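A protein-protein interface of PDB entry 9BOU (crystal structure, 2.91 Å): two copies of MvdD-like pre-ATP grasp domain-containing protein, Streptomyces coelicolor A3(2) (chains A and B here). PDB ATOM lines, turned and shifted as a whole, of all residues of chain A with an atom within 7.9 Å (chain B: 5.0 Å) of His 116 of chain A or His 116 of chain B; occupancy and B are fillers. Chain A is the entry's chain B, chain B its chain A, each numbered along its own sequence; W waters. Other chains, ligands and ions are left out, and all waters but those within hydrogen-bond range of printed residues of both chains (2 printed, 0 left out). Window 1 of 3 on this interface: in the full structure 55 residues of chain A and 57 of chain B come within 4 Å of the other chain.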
ATOM      1  N   GLN A  95      39.309  19.326   5.121  1.00  0.00           N
ATOM      2  CA  GLN A  95      38.669  20.592   4.782  1.00  0.00           C
ATOM      3  C   GLN A  95      39.552  21.431   3.871  1.00  0.00           C
ATOM      4  O   GLN A  95      39.117  21.890   2.807  1.00  0.00           O
ATOM      5  CB  GLN A  95      38.332  21.373   6.040  1.00  0.00           C
ATOM      6  CG  GLN A  95      37.275  20.696   6.823  1.00  0.00           C
ATOM      7  CD  GLN A  95      35.971  21.396   6.693  1.00  0.00           C
ATOM      8  OE1 GLN A  95      35.929  22.637   6.557  1.00  0.00           O
ATOM      9  NE2 GLN A  95      34.869  20.615   6.755  1.00  0.00           N
ATOM     10  N   TYR A  98      39.445  19.067   0.362  1.00  0.00           N
ATOM     11  CA  TYR A  98      38.200  18.896  -0.356  1.00  0.00           C
ATOM     12  C   TYR A  98      37.349  20.155  -0.394  1.00  0.00           C
ATOM     13  O   TYR A  98      36.348  20.203  -1.125  1.00  0.00           O
ATOM     14  CB  TYR A  98      37.452  17.748   0.286  1.00  0.00           C
ATOM     15  CG  TYR A  98      38.142  16.421   0.088  1.00  0.00           C
ATOM     16  CD1 TYR A  98      38.095  15.761  -1.137  1.00  0.00           C
ATOM     17  CD2 TYR A  98      38.841  15.808   1.135  1.00  0.00           C
ATOM     18  CE1 TYR A  98      38.722  14.525  -1.310  1.00  0.00           C
ATOM     19  CE2 TYR A  98      39.462  14.563   0.969  1.00  0.00           C
ATOM     20  CZ  TYR A  98      39.384  13.921  -0.258  1.00  0.00           C
ATOM     21  OH  TYR A  98      39.992  12.700  -0.415  1.00  0.00           O
ATOM     22  N   ARG A 102      36.411  21.970  -4.081  1.00  0.00           N
ATOM     23  CA  ARG A 102      35.026  22.349  -4.302  1.00  0.00           C
ATOM     24  C   ARG A 102      34.960  23.799  -4.769  1.00  0.00           C
ATOM     25  O   ARG A 102      35.448  24.718  -4.091  1.00  0.00           O
ATOM     26  CB  ARG A 102      34.266  22.156  -3.000  1.00  0.00           C
ATOM     27  CG  ARG A 102      33.450  20.896  -2.903  1.00  0.00           C
ATOM     28  CD  ARG A 102      32.589  20.929  -1.634  1.00  0.00           C
ATOM     29  NE  ARG A 102      32.082  19.644  -1.184  1.00  0.00           N
ATOM     30  CZ  ARG A 102      32.774  18.814  -0.423  1.00  0.00           C
ATOM     31  NH1 ARG A 102      34.033  19.068  -0.105  1.00  0.00           N
ATOM     32  NH2 ARG A 102      32.168  17.740   0.085  1.00  0.00           N
ATOM     33  N   ASN A 110      32.461  11.667  -9.588  1.00  0.00           N
ATOM     34  CA  ASN A 110      31.611  11.641  -8.404  1.00  0.00           C
ATOM     35  C   ASN A 110      32.019  12.791  -7.552  1.00  0.00           C
ATOM     36  O   ASN A 110      33.021  12.753  -6.873  1.00  0.00           O
ATOM     37  CB  ASN A 110      31.600  10.261  -7.826  1.00  0.00           C
ATOM     38  CG  ASN A 110      30.801   9.315  -8.743  1.00  0.00           C
ATOM     39  OD1 ASN A 110      30.517   9.670  -9.902  1.00  0.00           O
ATOM     40  ND2 ASN A 110      30.491   8.116  -8.250  1.00  0.00           N
ATOM     41  N   GLN A 111      31.261  13.853  -7.729  1.00  0.00           N
ATOM     42  CA  GLN A 111      31.322  15.003  -6.870  1.00  0.00           C
ATOM     43  C   GLN A 111      31.002  14.572  -5.441  1.00  0.00           C
ATOM     44  O   GLN A 111      30.026  13.840  -5.225  1.00  0.00           O
ATOM     45  CB  GLN A 111      30.333  16.046  -7.402  1.00  0.00           C
ATOM     46  CG  GLN A 111      30.619  17.438  -6.970  1.00  0.00           C
ATOM     47  CD  GLN A 111      29.921  17.737  -5.645  1.00  0.00           C
ATOM     48  OE1 GLN A 111      28.927  17.081  -5.314  1.00  0.00           O
ATOM     49  NE2 GLN A 111      30.448  18.678  -4.873  1.00  0.00           N
ATOM     50  N   PRO A 112      31.796  15.017  -4.449  1.00  0.00           N
ATOM     51  CA  PRO A 112      31.679  14.450  -3.101  1.00  0.00           C
ATOM     52  C   PRO A 112      30.284  14.477  -2.521  1.00  0.00           C
ATOM     53  O   PRO A 112      29.959  13.637  -1.670  1.00  0.00           O
ATOM     54  CB  PRO A 112      32.596  15.337  -2.243  1.00  0.00           C
ATOM     55  CG  PRO A 112      33.415  16.065  -3.198  1.00  0.00           C
ATOM     56  CD  PRO A 112      32.592  16.247  -4.425  1.00  0.00           C
ATOM     57  N   ASP A 113      29.452  15.438  -2.925  1.00  0.00           N
ATOM     58  CA  ASP A 113      28.147  15.680  -2.297  1.00  0.00           C
ATOM     59  C   ASP A 113      27.053  14.837  -2.920  1.00  0.00           C
ATOM     60  O   ASP A 113      26.277  14.206  -2.206  1.00  0.00           O
ATOM     61  CB  ASP A 113      27.878  17.188  -2.366  1.00  0.00           C
ATOM     62  CG  ASP A 113      29.029  18.003  -1.696  1.00  0.00           C
ATOM     63  OD1 ASP A 113      29.296  17.783  -0.491  1.00  0.00           O
ATOM     64  OD2 ASP A 113      29.692  18.827  -2.366  1.00  0.00           O
ATOM     65  N   ALA A 114      27.019  14.776  -4.242  1.00  0.00           N
ATOM     66  CA  ALA A 114      26.342  13.681  -4.923  1.00  0.00           C
ATOM     67  C   ALA A 114      26.726  12.336  -4.341  1.00  0.00           C
ATOM     68  O   ALA A 114      25.855  11.526  -3.974  1.00  0.00           O
ATOM     69  CB  ALA A 114      26.683  13.693  -6.410  1.00  0.00           C
ATOM     70  N   ALA A 115      28.033  12.074  -4.293  1.00  0.00           N
ATOM     71  CA  ALA A 115      28.533  10.821  -3.749  1.00  0.00           C
ATOM     72  C   ALA A 115      28.021  10.547  -2.331  1.00  0.00           C
ATOM     73  O   ALA A 115      27.588   9.423  -2.030  1.00  0.00           O
ATOM     74  CB  ALA A 115      30.057  10.832  -3.780  1.00  0.00           C
ATOM     75  N   HIS A 116      28.066  11.556  -1.443  1.00  0.00           N
ATOM     76  CA  HIS A 116      27.488  11.413  -0.103  1.00  0.00           C
ATOM     77  C   HIS A 116      26.035  10.916  -0.173  1.00  0.00           C
ATOM     78  O   HIS A 116      25.694   9.855   0.362  1.00  0.00           O
ATOM     79  CB  HIS A 116      27.578  12.753   0.663  1.00  0.00           C
ATOM     80  CG  HIS A 116      27.169  12.656   2.113  1.00  0.00           C
ATOM     81  ND1 HIS A 116      25.882  12.928   2.552  1.00  0.00           N
ATOM     82  CD2 HIS A 116      27.871  12.289   3.212  1.00  0.00           C
ATOM     83  CE1 HIS A 116      25.815  12.733   3.855  1.00  0.00           C
ATOM     84  NE2 HIS A 116      27.008  12.352   4.280  1.00  0.00           N
ATOM     85  N   ARG A 117      25.159  11.693  -0.825  1.00  0.00           N
ATOM     86  CA  ARG A 117      23.763  11.300  -1.005  1.00  0.00           C
ATOM     87  C   ARG A 117      23.606   9.899  -1.619  1.00  0.00           C
ATOM     88  O   ARG A 117      22.602   9.201  -1.367  1.00  0.00           O
ATOM     89  CB  ARG A 117      23.058  12.381  -1.859  1.00  0.00           C
ATOM     90  CG  ARG A 117      22.193  11.875  -2.934  1.00  0.00           C
ATOM     91  CD  ARG A 117      21.282  12.971  -3.611  1.00  0.00           C
ATOM     92  NE  ARG A 117      20.088  13.026  -2.803  1.00  0.00           N
ATOM     93  CZ  ARG A 117      18.978  13.652  -3.155  1.00  0.00           C
ATOM     94  NH1 ARG A 117      18.868  14.248  -4.330  1.00  0.00           N
ATOM     95  NH2 ARG A 117      17.962  13.699  -2.299  1.00  0.00           N
ATOM     96  N   ALA A 118      24.563   9.469  -2.431  1.00  0.00           N
ATOM     97  CA  ALA A 118      24.340   8.272  -3.225  1.00  0.00           C
ATOM     98  C   ALA A 118      24.605   6.997  -2.456  1.00  0.00           C
ATOM     99  O   ALA A 118      24.168   5.928  -2.890  1.00  0.00           O
ATOM    100  CB  ALA A 118      25.225   8.325  -4.456  1.00  0.00           C
ATOM    101  N   ARG A 119      25.316   7.078  -1.333  1.00  0.00           N
ATOM    102  CA  ARG A 119      25.566   5.881  -0.550  1.00  0.00           C
ATOM    103  C   ARG A 119      24.315   5.385   0.177  1.00  0.00           C
ATOM    104  O   ARG A 119      24.350   4.279   0.722  1.00  0.00           O
ATOM    105  CB  ARG A 119      26.717   6.144   0.425  1.00  0.00           C
ATOM    106  CG  ARG A 119      28.057   6.462  -0.259  1.00  0.00           C
ATOM    107  CD  ARG A 119      29.179   6.823   0.733  1.00  0.00           C
ATOM    108  NE  ARG A 119      30.200   7.684   0.135  1.00  0.00           N
ATOM    109  CZ  ARG A 119      30.644   8.834   0.655  1.00  0.00           C
ATOM    110  NH1 ARG A 119      30.164   9.324   1.794  1.00  0.00           N
ATOM    111  NH2 ARG A 119      31.597   9.512   0.014  1.00  0.00           N
ATOM    112  N   TYR A 120      23.203   6.127   0.150  1.00  0.00           N
ATOM    113  CA  TYR A 120      21.985   5.741   0.867  1.00  0.00           C
ATOM    114  C   TYR A 120      21.113   4.861  -0.019  1.00  0.00           C
ATOM    115  O   TYR A 120      20.342   5.359  -0.850  1.00  0.00           O
ATOM    116  CB  TYR A 120      21.199   6.971   1.316  1.00  0.00           C
ATOM    117  CG  TYR A 120      21.836   7.744   2.467  1.00  0.00           C
ATOM    118  CD1 TYR A 120      22.832   8.638   2.236  1.00  0.00           C
ATOM    119  CD2 TYR A 120      21.442   7.559   3.775  1.00  0.00           C
ATOM    120  CE1 TYR A 120      23.435   9.326   3.270  1.00  0.00           C
ATOM    121  CE2 TYR A 120      22.045   8.243   4.808  1.00  0.00           C
ATOM    122  CZ  TYR A 120      23.043   9.118   4.558  1.00  0.00           C
ATOM    123  OH  TYR A 120      23.664   9.835   5.575  1.00  0.00           O
ATOM    124  N   LYS A 121      21.196   3.548   0.203  1.00  0.00           N
ATOM    125  CA  LYS A 121      20.472   2.605  -0.638  1.00  0.00           C
ATOM    126  C   LYS A 121      18.965   2.801  -0.639  1.00  0.00           C
ATOM    127  O   LYS A 121      18.349   2.610  -1.706  1.00  0.00           O
ATOM    128  CB  LYS A 121      20.761   1.162  -0.213  1.00  0.00           C
ATOM    129  CG  LYS A 121      22.220   0.788  -0.168  1.00  0.00           C
ATOM    130  CD  LYS A 121      22.446  -0.732   0.101  1.00  0.00           C
ATOM    131  CE  LYS A 121      21.180  -1.638  -0.024  1.00  0.00           C
ATOM    132  NZ  LYS A 121      21.527  -3.036   0.365  1.00  0.00           N
ATOM    133  N   TRP A 123      17.437   5.512  -0.643  1.00  0.00           N
ATOM    134  CA  TRP A 123      17.263   6.565  -1.638  1.00  0.00           C
ATOM    135  C   TRP A 123      17.412   5.977  -3.036  1.00  0.00           C
ATOM    136  O   TRP A 123      16.538   6.172  -3.897  1.00  0.00           O
ATOM    137  CB  TRP A 123      18.226   7.736  -1.368  1.00  0.00           C
ATOM    138  CG  TRP A 123      18.323   8.648  -2.559  1.00  0.00           C
ATOM    139  CD1 TRP A 123      19.470   9.005  -3.228  1.00  0.00           C
ATOM    140  CD2 TRP A 123      17.255   9.277  -3.234  1.00  0.00           C
ATOM    141  NE1 TRP A 123      19.171   9.817  -4.286  1.00  0.00           N
ATOM    142  CE2 TRP A 123      17.815  10.008  -4.317  1.00  0.00           C
ATOM    143  CE3 TRP A 123      15.879   9.298  -3.050  1.00  0.00           C
ATOM    144  CZ2 TRP A 123      17.043  10.755  -5.206  1.00  0.00           C
ATOM    145  CZ3 TRP A 123      15.091  10.051  -3.948  1.00  0.00           C
ATOM    146  CH2 TRP A 123      15.684  10.761  -5.011  1.00  0.00           C
ATOM    147  N   GLY A 164      24.605   1.194   2.284  1.00  0.00           N
ATOM    148  CA  GLY A 164      25.570   1.300   1.193  1.00  0.00           C
ATOM    149  C   GLY A 164      26.769   2.197   1.543  1.00  0.00           C
ATOM    150  O   GLY A 164      27.653   1.828   2.362  1.00  0.00           O
ATOM    151  N   LEU A 263      25.821  11.750 -10.941  1.00  0.00           N
ATOM    152  CA  LEU A 263      26.986  10.882 -10.849  1.00  0.00           C
ATOM    153  C   LEU A 263      27.619  10.672 -12.225  1.00  0.00           C
ATOM    154  O   LEU A 263      26.929  10.386 -13.212  1.00  0.00           O
ATOM    155  CB  LEU A 263      26.607   9.539 -10.231  1.00  0.00           C
ATOM    156  CG  LEU A 263      26.161   9.579  -8.778  1.00  0.00           C
ATOM    157  CD1 LEU A 263      25.810   8.176  -8.332  1.00  0.00           C
ATOM    158  CD2 LEU A 263      27.248  10.144  -7.877  1.00  0.00           C
ATOM    159  N   GLN A 285      28.510   4.003  -6.171  1.00  0.00           N
ATOM    160  CA  GLN A 285      29.083   5.160  -6.863  1.00  0.00           C
ATOM    161  C   GLN A 285      30.610   5.053  -6.976  1.00  0.00           C
ATOM    162  O   GLN A 285      31.224   5.751  -7.799  1.00  0.00           O
ATOM    163  CB  GLN A 285      28.605   6.463  -6.158  1.00  0.00           C
ATOM    164  CG  GLN A 285      29.101   6.718  -4.749  1.00  0.00           C
ATOM    165  CD  GLN A 285      30.475   7.348  -4.735  1.00  0.00           C
ATOM    166  OE1 GLN A 285      30.889   7.964  -5.724  1.00  0.00           O
ATOM    167  NE2 GLN A 285      31.195   7.201  -3.624  1.00  0.00           N
ATOM    168  N   ARG B 102      14.807  11.095   2.259  1.00  0.00           N
ATOM    169  CA  ARG B 102      15.200  11.576   0.940  1.00  0.00           C
ATOM    170  C   ARG B 102      14.166  11.122  -0.096  1.00  0.00           C
ATOM    171  O   ARG B 102      13.787   9.941  -0.147  1.00  0.00           O
ATOM    172  CB  ARG B 102      16.604  11.058   0.609  1.00  0.00           C
ATOM    173  CG  ARG B 102      17.759  11.830   1.281  1.00  0.00           C
ATOM    174  CD  ARG B 102      19.066  11.042   1.165  1.00  0.00           C
ATOM    175  NE  ARG B 102      20.259  11.781   1.549  1.00  0.00           N
ATOM    176  CZ  ARG B 102      20.824  11.697   2.744  1.00  0.00           C
ATOM    177  NH1 ARG B 102      20.299  10.952   3.705  1.00  0.00           N
ATOM    178  NH2 ARG B 102      21.946  12.376   2.983  1.00  0.00           N
ATOM    179  N   PRO B 112      20.104  17.209   4.058  1.00  0.00           N
ATOM    180  CA  PRO B 112      21.332  16.673   4.679  1.00  0.00           C
ATOM    181  C   PRO B 112      22.555  16.738   3.794  1.00  0.00           C
ATOM    182  O   PRO B 112      23.679  16.773   4.316  1.00  0.00           O
ATOM    183  CB  PRO B 112      20.972  15.223   5.015  1.00  0.00           C
ATOM    184  CG  PRO B 112      19.577  15.024   4.503  1.00  0.00           C
ATOM    185  CD  PRO B 112      18.943  16.314   4.208  1.00  0.00           C
ATOM    186  N   ASP B 113      22.375  16.744   2.481  1.00  0.00           N
ATOM    187  CA  ASP B 113      23.468  16.805   1.521  1.00  0.00           C
ATOM    188  C   ASP B 113      23.926  18.233   1.270  1.00  0.00           C
ATOM    189  O   ASP B 113      25.132  18.479   1.185  1.00  0.00           O
ATOM    190  CB  ASP B 113      23.022  16.065   0.256  1.00  0.00           C
ATOM    191  CG  ASP B 113      22.569  14.679   0.578  1.00  0.00           C
ATOM    192  OD1 ASP B 113      23.326  13.985   1.292  1.00  0.00           O
ATOM    193  OD2 ASP B 113      21.436  14.274   0.197  1.00  0.00           O
ATOM    194  N   ALA B 114      23.006  19.186   1.182  1.00  0.00           N
ATOM    195  CA  ALA B 114      23.401  20.583   1.247  1.00  0.00           C
ATOM    196  C   ALA B 114      24.271  20.820   2.473  1.00  0.00           C
ATOM    197  O   ALA B 114      25.381  21.363   2.385  1.00  0.00           O
ATOM    198  CB  ALA B 114      22.142  21.454   1.296  1.00  0.00           C
ATOM    199  N   ALA B 115      23.761  20.386   3.621  1.00  0.00           N
ATOM    200  CA  ALA B 115      24.441  20.534   4.899  1.00  0.00           C
ATOM    201  C   ALA B 115      25.849  19.977   4.894  1.00  0.00           C
ATOM    202  O   ALA B 115      26.757  20.548   5.503  1.00  0.00           O
ATOM    203  CB  ALA B 115      23.616  19.809   5.960  1.00  0.00           C
ATOM    204  N   HIS B 116      26.038  18.825   4.272  1.00  0.00           N
ATOM    205  CA  HIS B 116      27.366  18.233   4.198  1.00  0.00           C
ATOM    206  C   HIS B 116      28.325  19.118   3.409  1.00  0.00           C
ATOM    207  O   HIS B 116      29.458  19.357   3.818  1.00  0.00           O
ATOM    208  CB  HIS B 116      27.256  16.842   3.567  1.00  0.00           C
ATOM    209  CG  HIS B 116      28.567  16.142   3.406  1.00  0.00           C
ATOM    210  ND1 HIS B 116      29.307  16.212   2.245  1.00  0.00           N
ATOM    211  CD2 HIS B 116      29.266  15.363   4.264  1.00  0.00           C
ATOM    212  CE1 HIS B 116      30.396  15.476   2.385  1.00  0.00           C
ATOM    213  NE2 HIS B 116      30.402  14.969   3.604  1.00  0.00           N
ATOM    214  N   ARG B 117      27.897  19.578   2.260  1.00  0.00           N
ATOM    215  CA  ARG B 117      28.728  20.483   1.507  1.00  0.00           C
ATOM    216  C   ARG B 117      28.945  21.786   2.257  1.00  0.00           C
ATOM    217  O   ARG B 117      29.989  22.420   2.126  1.00  0.00           O
ATOM    218  CB  ARG B 117      28.070  20.682   0.160  1.00  0.00           C
ATOM    219  CG  ARG B 117      28.475  21.939  -0.523  1.00  0.00           C
ATOM    220  CD  ARG B 117      27.940  21.875  -1.931  1.00  0.00           C
ATOM    221  NE  ARG B 117      29.041  22.182  -2.815  1.00  0.00           N
ATOM    222  CZ  ARG B 117      28.916  22.365  -4.112  1.00  0.00           C
ATOM    223  NH1 ARG B 117      27.758  22.157  -4.725  1.00  0.00           N
ATOM    224  NH2 ARG B 117      29.968  22.793  -4.799  1.00  0.00           N
ATOM    225  N   ALA B 118      27.997  22.191   3.068  1.00  0.00           N
ATOM    226  CA  ALA B 118      28.072  23.519   3.643  1.00  0.00           C
ATOM    227  C   ALA B 118      29.031  23.604   4.813  1.00  0.00           C
ATOM    228  O   ALA B 118      29.391  24.715   5.208  1.00  0.00           O
ATOM    229  CB  ALA B 118      26.664  23.959   4.064  1.00  0.00           C
ATOM    230  N   ARG B 119      29.430  22.471   5.393  1.00  0.00           N
ATOM    231  CA  ARG B 119      30.351  22.504   6.518  1.00  0.00           C
ATOM    232  C   ARG B 119      31.767  22.787   6.084  1.00  0.00           C
ATOM    233  O   ARG B 119      32.639  22.973   6.939  1.00  0.00           O
ATOM    234  CB  ARG B 119      30.362  21.187   7.273  1.00  0.00           C
ATOM    235  CG  ARG B 119      29.007  20.787   7.711  1.00  0.00           C
ATOM    236  CD  ARG B 119      29.076  19.783   8.828  1.00  0.00           C
ATOM    237  NE  ARG B 119      27.786  19.108   8.884  1.00  0.00           N
ATOM    238  CZ  ARG B 119      27.584  17.836   8.561  1.00  0.00           C
ATOM    239  NH1 ARG B 119      28.595  17.020   8.253  1.00  0.00           N
ATOM    240  NH2 ARG B 119      26.337  17.369   8.534  1.00  0.00           N
ATOM    241  N   TYR B 120      32.020  22.772   4.785  1.00  0.00           N
ATOM    242  CA  TYR B 120      33.377  22.904   4.271  1.00  0.00           C
ATOM    243  C   TYR B 120      33.712  24.382   4.208  1.00  0.00           C
ATOM    244  O   TYR B 120      33.453  25.065   3.222  1.00  0.00           O
ATOM    245  CB  TYR B 120      33.497  22.206   2.937  1.00  0.00           C
ATOM    246  CG  TYR B 120      33.779  20.725   3.110  1.00  0.00           C
ATOM    247  CD1 TYR B 120      35.055  20.268   3.322  1.00  0.00           C
ATOM    248  CD2 TYR B 120      32.755  19.782   3.048  1.00  0.00           C
ATOM    249  CE1 TYR B 120      35.309  18.912   3.469  1.00  0.00           C
ATOM    250  CE2 TYR B 120      33.005  18.415   3.190  1.00  0.00           C
ATOM    251  CZ  TYR B 120      34.267  17.992   3.408  1.00  0.00           C
ATOM    252  OH  TYR B 120      34.549  16.647   3.561  1.00  0.00           O
HETATM  253  O   HOH W   1      22.660  12.196   6.112  1.00  0.00           O
HETATM  254  O   HOH W   2      33.861  15.510   1.203  1.00  0.00           O
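His 116 of chain B touches three residues of chain A. No residue of chain A comes within 4 Å of Ala 115 of chain B. Printed residues of chain A within 4 Å of Arg 102 of chain B: His 116, Tyr 120 and Trp 123. Printed residues of chain A within 4 Å of Asp 113 of chain B: His 116 and Arg 117. Of the printed residues of chain B, Asp 113 of chain A touches His 116 and Arg 117.
A ring nitrogen (ND1) of His 116 of chain B lies within hydrogen-bond range of the side-chain carboxylate (OD1) of Asp 113 of chain A (3.2 Å). NE of Arg 117 of chain A is in salt-bridge range of OD2 of Asp 113 of chain B, at 3.5 Å. OD2 of Asp 113 of chain A is in salt-bridge range of NE of Arg 117 of chain B (3.4 Å). OD1 of Asp 113 of chain B sits at hydrogen-bond distance from ND1 of His 116 of chain A. NE2 of Gln 95 of chain A is in hydrogen-bond range of O of Arg 119 of chain B (3.3 Å).
Water W1 bridges the side-chain hydroxyl of Tyr 120 of chain A (2.6 Å) and the guanidinium group of Arg 102 of chain B (3.2 Å). Water W2 lies within hydrogen-bond range of OH of Tyr 120 of chain B and NH2 of Arg 102 of chain A.
Of the 19 printed residues of chain A, 7 touch a printed residue of chain B. Hydrophobic or aromatic side chains of chain A that line the printed part of chain B: His 116, Tyr 120 and Trp 123. Among the printed residues, 13 pairs touch across the chains. Among the printed residues, Asp or Glu carboxylates within 4 Å of a Lys or Arg side-chain nitrogen of the other chain: Asp 113 of chain A with Arg 117 of chain B (3.4 Å) and Arg 117 of chain A with Asp 113 of chain B (3.5 Å).
Arg 102 of chain A touches His 116 of chain B, and with the chains exchanged His 116 of chain A touches Arg 102 of chain B. Arg 102 of chain A touches Arg 117 of chain B, but with the chains exchanged Arg 117 of chain A does not touch Arg 102 of chain B (4.04 Å). Arg 102 of chain A touches Tyr 120 of chain B, and with the chains exchanged Tyr 120 of chain A touches Arg 102 of chain B. Asp 113 of chain A touches Arg 117 of chain B, and with the chains exchanged Arg 117 of chain A touches Asp 113 of chain B. 10 positions are printed for both chains. Of the 13 pairs that touch across the chains among the printed residues, 9 have their exchanged pair printed and touching as well.
NH1 of Arg 102 of chain A lies within hydrogen-bond range of O of Tyr 98 of chain A, at 2.8 Å. NE2 of Gln 111 of chain A lies within hydrogen-bond range of OD2 of Asp 113 of chain A, 2.6 Å away. The guanidinium group (NE) of Arg 102 of chain A is in salt-bridge range of the side-chain carboxylate (OD2) of Asp 113 of chain A (2.8 Å). The guanidinium group (NH2) of Arg 102 of chain B is in salt-bridge range of the side-chain carboxylate (OD1) of Asp 113 of chain B (2.7 Å).
Among the printed residues, merely in contact across the chains: Gln 95 of chain A with Tyr 120 of chain B (3.4 Å), Arg 102 of chain A with His 116 of chain B (3.7 Å), Arg 102 of chain A with Arg 117 of chain B (3.9 Å), Arg 102 of chain A with Tyr 120 of chain B (3.3 Å), His 116 of chain A with Arg 102 of chain B (3.98 Å), His 116 of chain A with His 116 of chain B (3.5 Å), Tyr 120 of chain A with Arg 102 of chain B (3.4 Å) and Trp 123 of chain A with Arg 102 of chain B (3.6 Å).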
